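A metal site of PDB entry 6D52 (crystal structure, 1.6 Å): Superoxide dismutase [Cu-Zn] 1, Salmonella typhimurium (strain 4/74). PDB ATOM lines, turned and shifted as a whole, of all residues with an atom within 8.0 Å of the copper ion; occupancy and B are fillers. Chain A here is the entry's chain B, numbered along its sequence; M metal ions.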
ATOM      1  N   GLY A  47       8.277   6.200   5.566  1.00  0.00           N
ATOM      2  CA  GLY A  47       8.734   5.014   4.857  1.00  0.00           C
ATOM      3  C   GLY A  47       7.934   3.806   5.281  1.00  0.00           C
ATOM      4  O   GLY A  47       7.734   3.561   6.472  1.00  0.00           O
ATOM      5  N   PHE A  48       7.472   3.029   4.296  1.00  0.00           N
ATOM      6  CA  PHE A  48       6.557   1.910   4.530  1.00  0.00           C
ATOM      7  C   PHE A  48       6.967   0.816   3.558  1.00  0.00           C
ATOM      8  O   PHE A  48       6.888   1.011   2.344  1.00  0.00           O
ATOM      9  CB  PHE A  48       5.121   2.405   4.299  1.00  0.00           C
ATOM     10  CG  PHE A  48       4.043   1.364   4.460  1.00  0.00           C
ATOM     11  CD1 PHE A  48       4.021   0.530   5.555  1.00  0.00           C
ATOM     12  CD2 PHE A  48       2.986   1.282   3.548  1.00  0.00           C
ATOM     13  CE1 PHE A  48       3.018  -0.403   5.710  1.00  0.00           C
ATOM     14  CE2 PHE A  48       1.982   0.343   3.696  1.00  0.00           C
ATOM     15  CZ  PHE A  48       1.990  -0.484   4.805  1.00  0.00           C
ATOM     16  N   HIS A  49       7.449  -0.314   4.068  1.00  0.00           N
ATOM     17  CA  HIS A  49       7.945  -1.370   3.184  1.00  0.00           C
ATOM     18  C   HIS A  49       7.692  -2.741   3.787  1.00  0.00           C
ATOM     19  O   HIS A  49       7.553  -2.904   5.013  1.00  0.00           O
ATOM     20  CB  HIS A  49       9.450  -1.263   2.917  1.00  0.00           C
ATOM     21  CG  HIS A  49       9.998   0.129   3.008  1.00  0.00           C
ATOM     22  ND1 HIS A  49      10.741   0.575   4.064  1.00  0.00           N
ATOM     23  CD2 HIS A  49       9.890   1.184   2.161  1.00  0.00           C
ATOM     24  CE1 HIS A  49      11.118   1.819   3.868  1.00  0.00           C
ATOM     25  NE2 HIS A  49      10.596   2.213   2.715  1.00  0.00           N
ATOM     26  N   VAL A  50       7.624  -3.727   2.901  1.00  0.00           N
ATOM     27  CA  VAL A  50       7.673  -5.126   3.305  1.00  0.00           C
ATOM     28  C   VAL A  50       9.121  -5.507   3.510  1.00  0.00           C
ATOM     29  O   VAL A  50       9.959  -5.292   2.620  1.00  0.00           O
ATOM     30  CB  VAL A  50       7.010  -6.036   2.263  1.00  0.00           C
ATOM     31  CG1 VAL A  50       6.861  -7.461   2.858  1.00  0.00           C
ATOM     32  CG2 VAL A  50       5.679  -5.509   1.797  1.00  0.00           C
ATOM     33  N   HIS A  51       9.421  -6.086   4.660  1.00  0.00           N
ATOM     34  CA  HIS A  51      10.762  -6.581   4.980  1.00  0.00           C
ATOM     35  C   HIS A  51      10.761  -8.108   4.985  1.00  0.00           C
ATOM     36  O   HIS A  51       9.713  -8.756   5.098  1.00  0.00           O
ATOM     37  CB  HIS A  51      11.246  -6.037   6.314  1.00  0.00           C
ATOM     38  CG  HIS A  51      11.647  -4.598   6.276  1.00  0.00           C
ATOM     39  ND1 HIS A  51      12.886  -4.159   6.666  1.00  0.00           N
ATOM     40  CD2 HIS A  51      10.984  -3.497   5.856  1.00  0.00           C
ATOM     41  CE1 HIS A  51      12.965  -2.850   6.535  1.00  0.00           C
ATOM     42  NE2 HIS A  51      11.823  -2.419   6.028  1.00  0.00           N
ATOM     43  N   ALA A  71      13.649  -7.970  11.453  1.00  0.00           N
ATOM     44  CA  ALA A  71      12.882  -8.044  10.224  1.00  0.00           C
ATOM     45  C   ALA A  71      13.768  -8.138   8.991  1.00  0.00           C
ATOM     46  O   ALA A  71      13.268  -8.439   7.903  1.00  0.00           O
ATOM     47  CB  ALA A  71      11.966  -6.814  10.094  1.00  0.00           C
ATOM     48  N   GLY A  72      15.066  -7.888   9.118  1.00  0.00           N
ATOM     49  CA  GLY A  72      15.883  -7.896   7.914  1.00  0.00           C
ATOM     50  C   GLY A  72      15.646  -6.670   7.053  1.00  0.00           C
ATOM     51  O   GLY A  72      15.113  -5.656   7.494  1.00  0.00           O
ATOM     52  N   GLY A  73      16.082  -6.774   5.804  1.00  0.00           N
ATOM     53  CA  GLY A  73      16.014  -5.678   4.866  1.00  0.00           C
ATOM     54  C   GLY A  73      14.722  -5.661   4.087  1.00  0.00           C
ATOM     55  O   GLY A  73      13.798  -6.423   4.328  1.00  0.00           O
ATOM     56  N   HIS A  74      14.674  -4.776   3.097  1.00  0.00           N
ATOM     57  CA  HIS A  74      13.511  -4.709   2.215  1.00  0.00           C
ATOM     58  C   HIS A  74      13.372  -5.982   1.381  1.00  0.00           C
ATOM     59  O   HIS A  74      14.354  -6.509   0.831  1.00  0.00           O
ATOM     60  CB  HIS A  74      13.596  -3.509   1.274  1.00  0.00           C
ATOM     61  CG  HIS A  74      13.637  -2.195   1.975  1.00  0.00           C
ATOM     62  ND1 HIS A  74      13.449  -0.993   1.323  1.00  0.00           N
ATOM     63  CD2 HIS A  74      13.833  -1.878   3.289  1.00  0.00           C
ATOM     64  CE1 HIS A  74      13.540  -0.003   2.188  1.00  0.00           C
ATOM     65  NE2 HIS A  74      13.788  -0.515   3.382  1.00  0.00           N
ATOM     66  N   LEU A  75      12.142  -6.487   1.291  1.00  0.00           N
ATOM     67  CA  LEU A  75      11.862  -7.671   0.511  1.00  0.00           C
ATOM     68  C   LEU A  75      12.332  -7.473  -0.924  1.00  0.00           C
ATOM     69  O   LEU A  75      11.981  -6.482  -1.579  1.00  0.00           O
ATOM     70  CB  LEU A  75      10.374  -7.988   0.556  1.00  0.00           C
ATOM     71  CG  LEU A  75       9.853  -9.153  -0.281  1.00  0.00           C
ATOM     72  CD1 LEU A  75      10.368 -10.498   0.235  1.00  0.00           C
ATOM     73  CD2 LEU A  75       8.332  -9.125  -0.298  1.00  0.00           C
ATOM     74  N   HIS A  83      16.651   0.535  -4.049  1.00  0.00           N
ATOM     75  CA  HIS A  83      15.403   1.065  -3.508  1.00  0.00           C
ATOM     76  C   HIS A  83      14.824   2.076  -4.489  1.00  0.00           C
ATOM     77  O   HIS A  83      15.319   3.208  -4.586  1.00  0.00           O
ATOM     78  CB  HIS A  83      15.629   1.691  -2.134  1.00  0.00           C
ATOM     79  CG  HIS A  83      14.378   2.217  -1.517  1.00  0.00           C
ATOM     80  ND1 HIS A  83      13.458   1.410  -0.867  1.00  0.00           N
ATOM     81  CD2 HIS A  83      13.854   3.469  -1.492  1.00  0.00           C
ATOM     82  CE1 HIS A  83      12.440   2.151  -0.476  1.00  0.00           C
ATOM     83  NE2 HIS A  83      12.646   3.396  -0.851  1.00  0.00           N
ATOM     84  N   HIS A  92      13.451  -3.003  -5.023  1.00  0.00           N
ATOM     85  CA  HIS A  92      12.879  -3.951  -4.079  1.00  0.00           C
ATOM     86  C   HIS A  92      11.389  -4.131  -4.293  1.00  0.00           C
ATOM     87  O   HIS A  92      10.639  -3.154  -4.281  1.00  0.00           O
ATOM     88  CB  HIS A  92      13.065  -3.467  -2.643  1.00  0.00           C
ATOM     89  CG  HIS A  92      14.448  -3.036  -2.287  1.00  0.00           C
ATOM     90  ND1 HIS A  92      14.696  -1.871  -1.594  1.00  0.00           N
ATOM     91  CD2 HIS A  92      15.643  -3.647  -2.458  1.00  0.00           C
ATOM     92  CE1 HIS A  92      15.995  -1.772  -1.363  1.00  0.00           C
ATOM     93  NE2 HIS A  92      16.598  -2.833  -1.885  1.00  0.00           N
ATOM     94  N   GLY A  94       9.438  -5.179  -2.100  1.00  0.00           N
ATOM     95  CA  GLY A  94       8.777  -4.784  -0.879  1.00  0.00           C
ATOM     96  C   GLY A  94       8.532  -3.304  -0.707  1.00  0.00           C
ATOM     97  O   GLY A  94       7.985  -2.902   0.316  1.00  0.00           O
ATOM     98  N   ASP A  95       8.925  -2.485  -1.689  1.00  0.00           N
ATOM     99  CA  ASP A  95       8.778  -1.028  -1.597  1.00  0.00           C
ATOM    100  C   ASP A  95       7.322  -0.620  -1.797  1.00  0.00           C
ATOM    101  O   ASP A  95       6.774  -0.739  -2.898  1.00  0.00           O
ATOM    102  CB  ASP A  95       9.679  -0.342  -2.632  1.00  0.00           C
ATOM    103  CG  ASP A  95      11.149  -0.443  -2.297  1.00  0.00           C
ATOM    104  OD1 ASP A  95      11.501  -0.918  -1.173  1.00  0.00           O
ATOM    105  OD2 ASP A  95      11.954  -0.048  -3.158  1.00  0.00           O
ATOM    106  N   LEU A  96       6.680  -0.148  -0.739  1.00  0.00           N
ATOM    107  CA  LEU A  96       5.303   0.302  -0.799  1.00  0.00           C
ATOM    108  C   LEU A  96       5.250   1.810  -0.886  1.00  0.00           C
ATOM    109  O   LEU A  96       6.235   2.500  -0.620  1.00  0.00           O
ATOM    110  CB  LEU A  96       4.556  -0.191   0.442  1.00  0.00           C
ATOM    111  CG  LEU A  96       4.698  -1.671   0.739  1.00  0.00           C
ATOM    112  CD1 LEU A  96       3.947  -2.013   2.017  1.00  0.00           C
ATOM    113  CD2 LEU A  96       4.177  -2.538  -0.429  1.00  0.00           C
ATOM    114  N   SER A 126       7.258  -9.128   6.943  1.00  0.00           N
ATOM    115  CA  SER A 126       6.830  -8.147   7.930  1.00  0.00           C
ATOM    116  C   SER A 126       6.537  -6.836   7.221  1.00  0.00           C
ATOM    117  O   SER A 126       7.036  -6.567   6.133  1.00  0.00           O
ATOM    118  CB  SER A 126       7.888  -7.947   9.009  1.00  0.00           C
ATOM    119  OG  SER A 126       9.166  -7.713   8.452  1.00  0.00           O
ATOM    120  N   LEU A 127       5.710  -6.023   7.858  1.00  0.00           N
ATOM    121  CA  LEU A 127       5.444  -4.665   7.393  1.00  0.00           C
ATOM    122  C   LEU A 127       6.124  -3.687   8.324  1.00  0.00           C
ATOM    123  O   LEU A 127       6.012  -3.826   9.550  1.00  0.00           O
ATOM    124  CB  LEU A 127       3.945  -4.340   7.352  1.00  0.00           C
ATOM    125  CG  LEU A 127       3.061  -5.152   6.425  1.00  0.00           C
ATOM    126  CD1 LEU A 127       1.674  -4.515   6.356  1.00  0.00           C
ATOM    127  CD2 LEU A 127       3.695  -5.289   5.030  1.00  0.00           C
ATOM    128  N   MET A 128       6.808  -2.692   7.763  1.00  0.00           N
ATOM    129  CA  MET A 128       7.626  -1.763   8.519  1.00  0.00           C
ATOM    130  C   MET A 128       7.197  -0.332   8.268  1.00  0.00           C
ATOM    131  O   MET A 128       7.000   0.056   7.114  1.00  0.00           O
ATOM    132  CB  MET A 128       9.102  -1.899   8.156  1.00  0.00           C
ATOM    133  CG  MET A 128      10.035  -1.251   9.134  1.00  0.00           C
ATOM    134  SD  MET A 128      10.138  -2.201  10.668  1.00  0.00           S
ATOM    135  CE  MET A 128      10.854  -3.714  10.099  1.00  0.00           C
ATOM    136  N   ILE A 129       7.041   0.438   9.352  1.00  0.00           N
ATOM    137  CA  ILE A 129       6.845   1.889   9.276  1.00  0.00           C
ATOM    138  C   ILE A 129       8.079   2.553   9.857  1.00  0.00           C
ATOM    139  O   ILE A 129       8.464   2.267  11.003  1.00  0.00           O
ATOM    140  CB  ILE A 129       5.580   2.331  10.019  1.00  0.00           C
ATOM    141  CG1 ILE A 129       4.354   1.637   9.451  1.00  0.00           C
ATOM    142  CG2 ILE A 129       5.413   3.846   9.932  1.00  0.00           C
ATOM    143  CD1 ILE A 129       3.092   1.802  10.293  1.00  0.00           C
ATOM    144  N   HIS A 130       8.710   3.420   9.078  1.00  0.00           N
ATOM    145  CA  HIS A 130       9.934   4.090   9.501  1.00  0.00           C
ATOM    146  C   HIS A 130       9.671   5.462  10.106  1.00  0.00           C
ATOM    147  O   HIS A 130       8.593   6.051   9.981  1.00  0.00           O
ATOM    148  CB  HIS A 130      10.899   4.226   8.311  1.00  0.00           C
ATOM    149  CG  HIS A 130      11.435   2.928   7.822  1.00  0.00           C
ATOM    150  ND1 HIS A 130      12.688   2.462   8.160  1.00  0.00           N
ATOM    151  CD2 HIS A 130      10.868   1.954   7.062  1.00  0.00           C
ATOM    152  CE1 HIS A 130      12.885   1.290   7.585  1.00  0.00           C
ATOM    153  NE2 HIS A 130      11.787   0.944   6.936  1.00  0.00           N
ATOM    154  N   ASP A 134      10.063   8.642   2.503  1.00  0.00           N
ATOM    155  CA  ASP A 134      10.522   7.792   1.411  1.00  0.00           C
ATOM    156  C   ASP A 134      10.409   8.555   0.103  1.00  0.00           C
ATOM    157  O   ASP A 134       9.301   8.810  -0.367  1.00  0.00           O
ATOM    158  CB  ASP A 134       9.699   6.505   1.370  1.00  0.00           C
ATOM    159  CG  ASP A 134      10.309   5.441   0.484  1.00  0.00           C
ATOM    160  OD1 ASP A 134      11.255   5.762  -0.276  1.00  0.00           O
ATOM    161  OD2 ASP A 134       9.876   4.263   0.571  1.00  0.00           O
ATOM    162  N   LEU A 143      17.833   3.834   0.876  1.00  0.00           N
ATOM    163  CA  LEU A 143      16.545   3.235   1.241  1.00  0.00           C
ATOM    164  C   LEU A 143      15.472   4.306   1.421  1.00  0.00           C
ATOM    165  O   LEU A 143      14.599   4.196   2.286  1.00  0.00           O
ATOM    166  CB  LEU A 143      16.695   2.379   2.506  1.00  0.00           C
ATOM    167  CG  LEU A 143      17.766   1.307   2.426  1.00  0.00           C
ATOM    168  CD1 LEU A 143      17.973   0.618   3.799  1.00  0.00           C
ATOM    169  CD2 LEU A 143      17.424   0.277   1.381  1.00  0.00           C
ATOM    170  N   GLY A 146      14.227   6.445   4.958  1.00  0.00           N
ATOM    171  CA  GLY A 146      13.352   5.981   6.026  1.00  0.00           C
ATOM    172  C   GLY A 146      14.044   5.953   7.368  1.00  0.00           C
ATOM    173  O   GLY A 146      13.421   6.208   8.408  1.00  0.00           O
ATOM    174  N   GLY A 147      15.340   5.656   7.379  1.00  0.00           N
ATOM    175  CA  GLY A 147      16.039   5.686   8.649  1.00  0.00           C
ATOM    176  C   GLY A 147      15.523   4.634   9.615  1.00  0.00           C
ATOM    177  O   GLY A 147      15.232   3.499   9.224  1.00  0.00           O
ATOM    178  N   ALA A 148      15.374   5.025  10.881  1.00  0.00           N
ATOM    179  CA  ALA A 148      15.058   4.069  11.938  1.00  0.00           C
ATOM    180  C   ALA A 148      13.652   3.482  11.766  1.00  0.00           C
ATOM    181  O   ALA A 148      12.771   4.065  11.117  1.00  0.00           O
ATOM    182  CB  ALA A 148      15.141   4.739  13.312  1.00  0.00           C
ATOM    183  N   ARG A 149      13.465   2.314  12.372  1.00  0.00           N
ATOM    184  CA  ARG A 149      12.219   1.574  12.317  1.00  0.00           C
ATOM    185  C   ARG A 149      11.364   1.944  13.528  1.00  0.00           C
ATOM    186  O   ARG A 149      11.806   1.782  14.669  1.00  0.00           O
ATOM    187  CB  ARG A 149      12.527   0.065  12.272  1.00  0.00           C
ATOM    188  CG  ARG A 149      13.449  -0.255  11.126  1.00  0.00           C
ATOM    189  CD  ARG A 149      14.007  -1.680  11.121  1.00  0.00           C
ATOM    190  NE  ARG A 149      14.867  -1.823   9.954  1.00  0.00           N
ATOM    191  CZ  ARG A 149      15.259  -2.963   9.396  1.00  0.00           C
ATOM    192  NH1 ARG A 149      14.897  -4.145   9.908  1.00  0.00           N
ATOM    193  NH2 ARG A 149      16.038  -2.905   8.318  1.00  0.00           N
ATOM    194  N   ALA A 151       7.572   1.312  13.788  1.00  0.00           N
ATOM    195  CA  ALA A 151       6.524   0.349  14.093  1.00  0.00           C
ATOM    196  C   ALA A 151       6.591  -0.761  13.076  1.00  0.00           C
ATOM    197  O   ALA A 151       7.139  -0.602  11.972  1.00  0.00           O
ATOM    198  CB  ALA A 151       5.133   0.975  14.133  1.00  0.00           C
HETATM  199 CU    CU M   1      11.441  -0.533   5.552  1.00  0.00          CU
HETATM  200 ZN    ZN M   2      13.348  -0.639  -0.687  1.00  0.00          ZN
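A ring nitrogen (ND1) of His 51 lies within hydrogen-bond range of the backbone carbonyl oxygen (O) of Gly 72, 2.8 Å away.
The backbone NH (N) of His 51 sits at hydrogen-bond distance from the backbone carbonyl oxygen (O) of Ser 126.
The backbone carbonyl oxygen of Gly 73 lies close to a ring nitrogen (ND1) of His 51, 3.4 Å away.
The backbone NH of His 130 is in hydrogen-bond range of the backbone carbonyl oxygen of Gly 47 (2.8 Å).
The backbone carbonyl oxygen (O) of Ala 148 lies close to a ring nitrogen (ND1) of His 130 (3.4 Å).
O of Gly 147 is in hydrogen-bond range of ND1 of His 130 (2.9 Å).
N of Met 128 is in hydrogen-bond range of O of His 49 (2.9 Å).
A ring nitrogen (ND1) of His 49 sits close to a ring nitrogen (NE2) of His 74 (3.3 Å).
Residues that only touch the copper ion: His 74 and Met 128.
Within 4 Å of the copper ion: His 49, His 51, His 74, Met 128 and His 130.
The nearest printed residue that does not touch the copper ion is Phe 48 (5.1 Å).
The copper ion is bound by a ring nitrogen (ND1) of His 49, a ring nitrogen (NE2) of His 51 and a ring nitrogen (NE2) of His 130.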
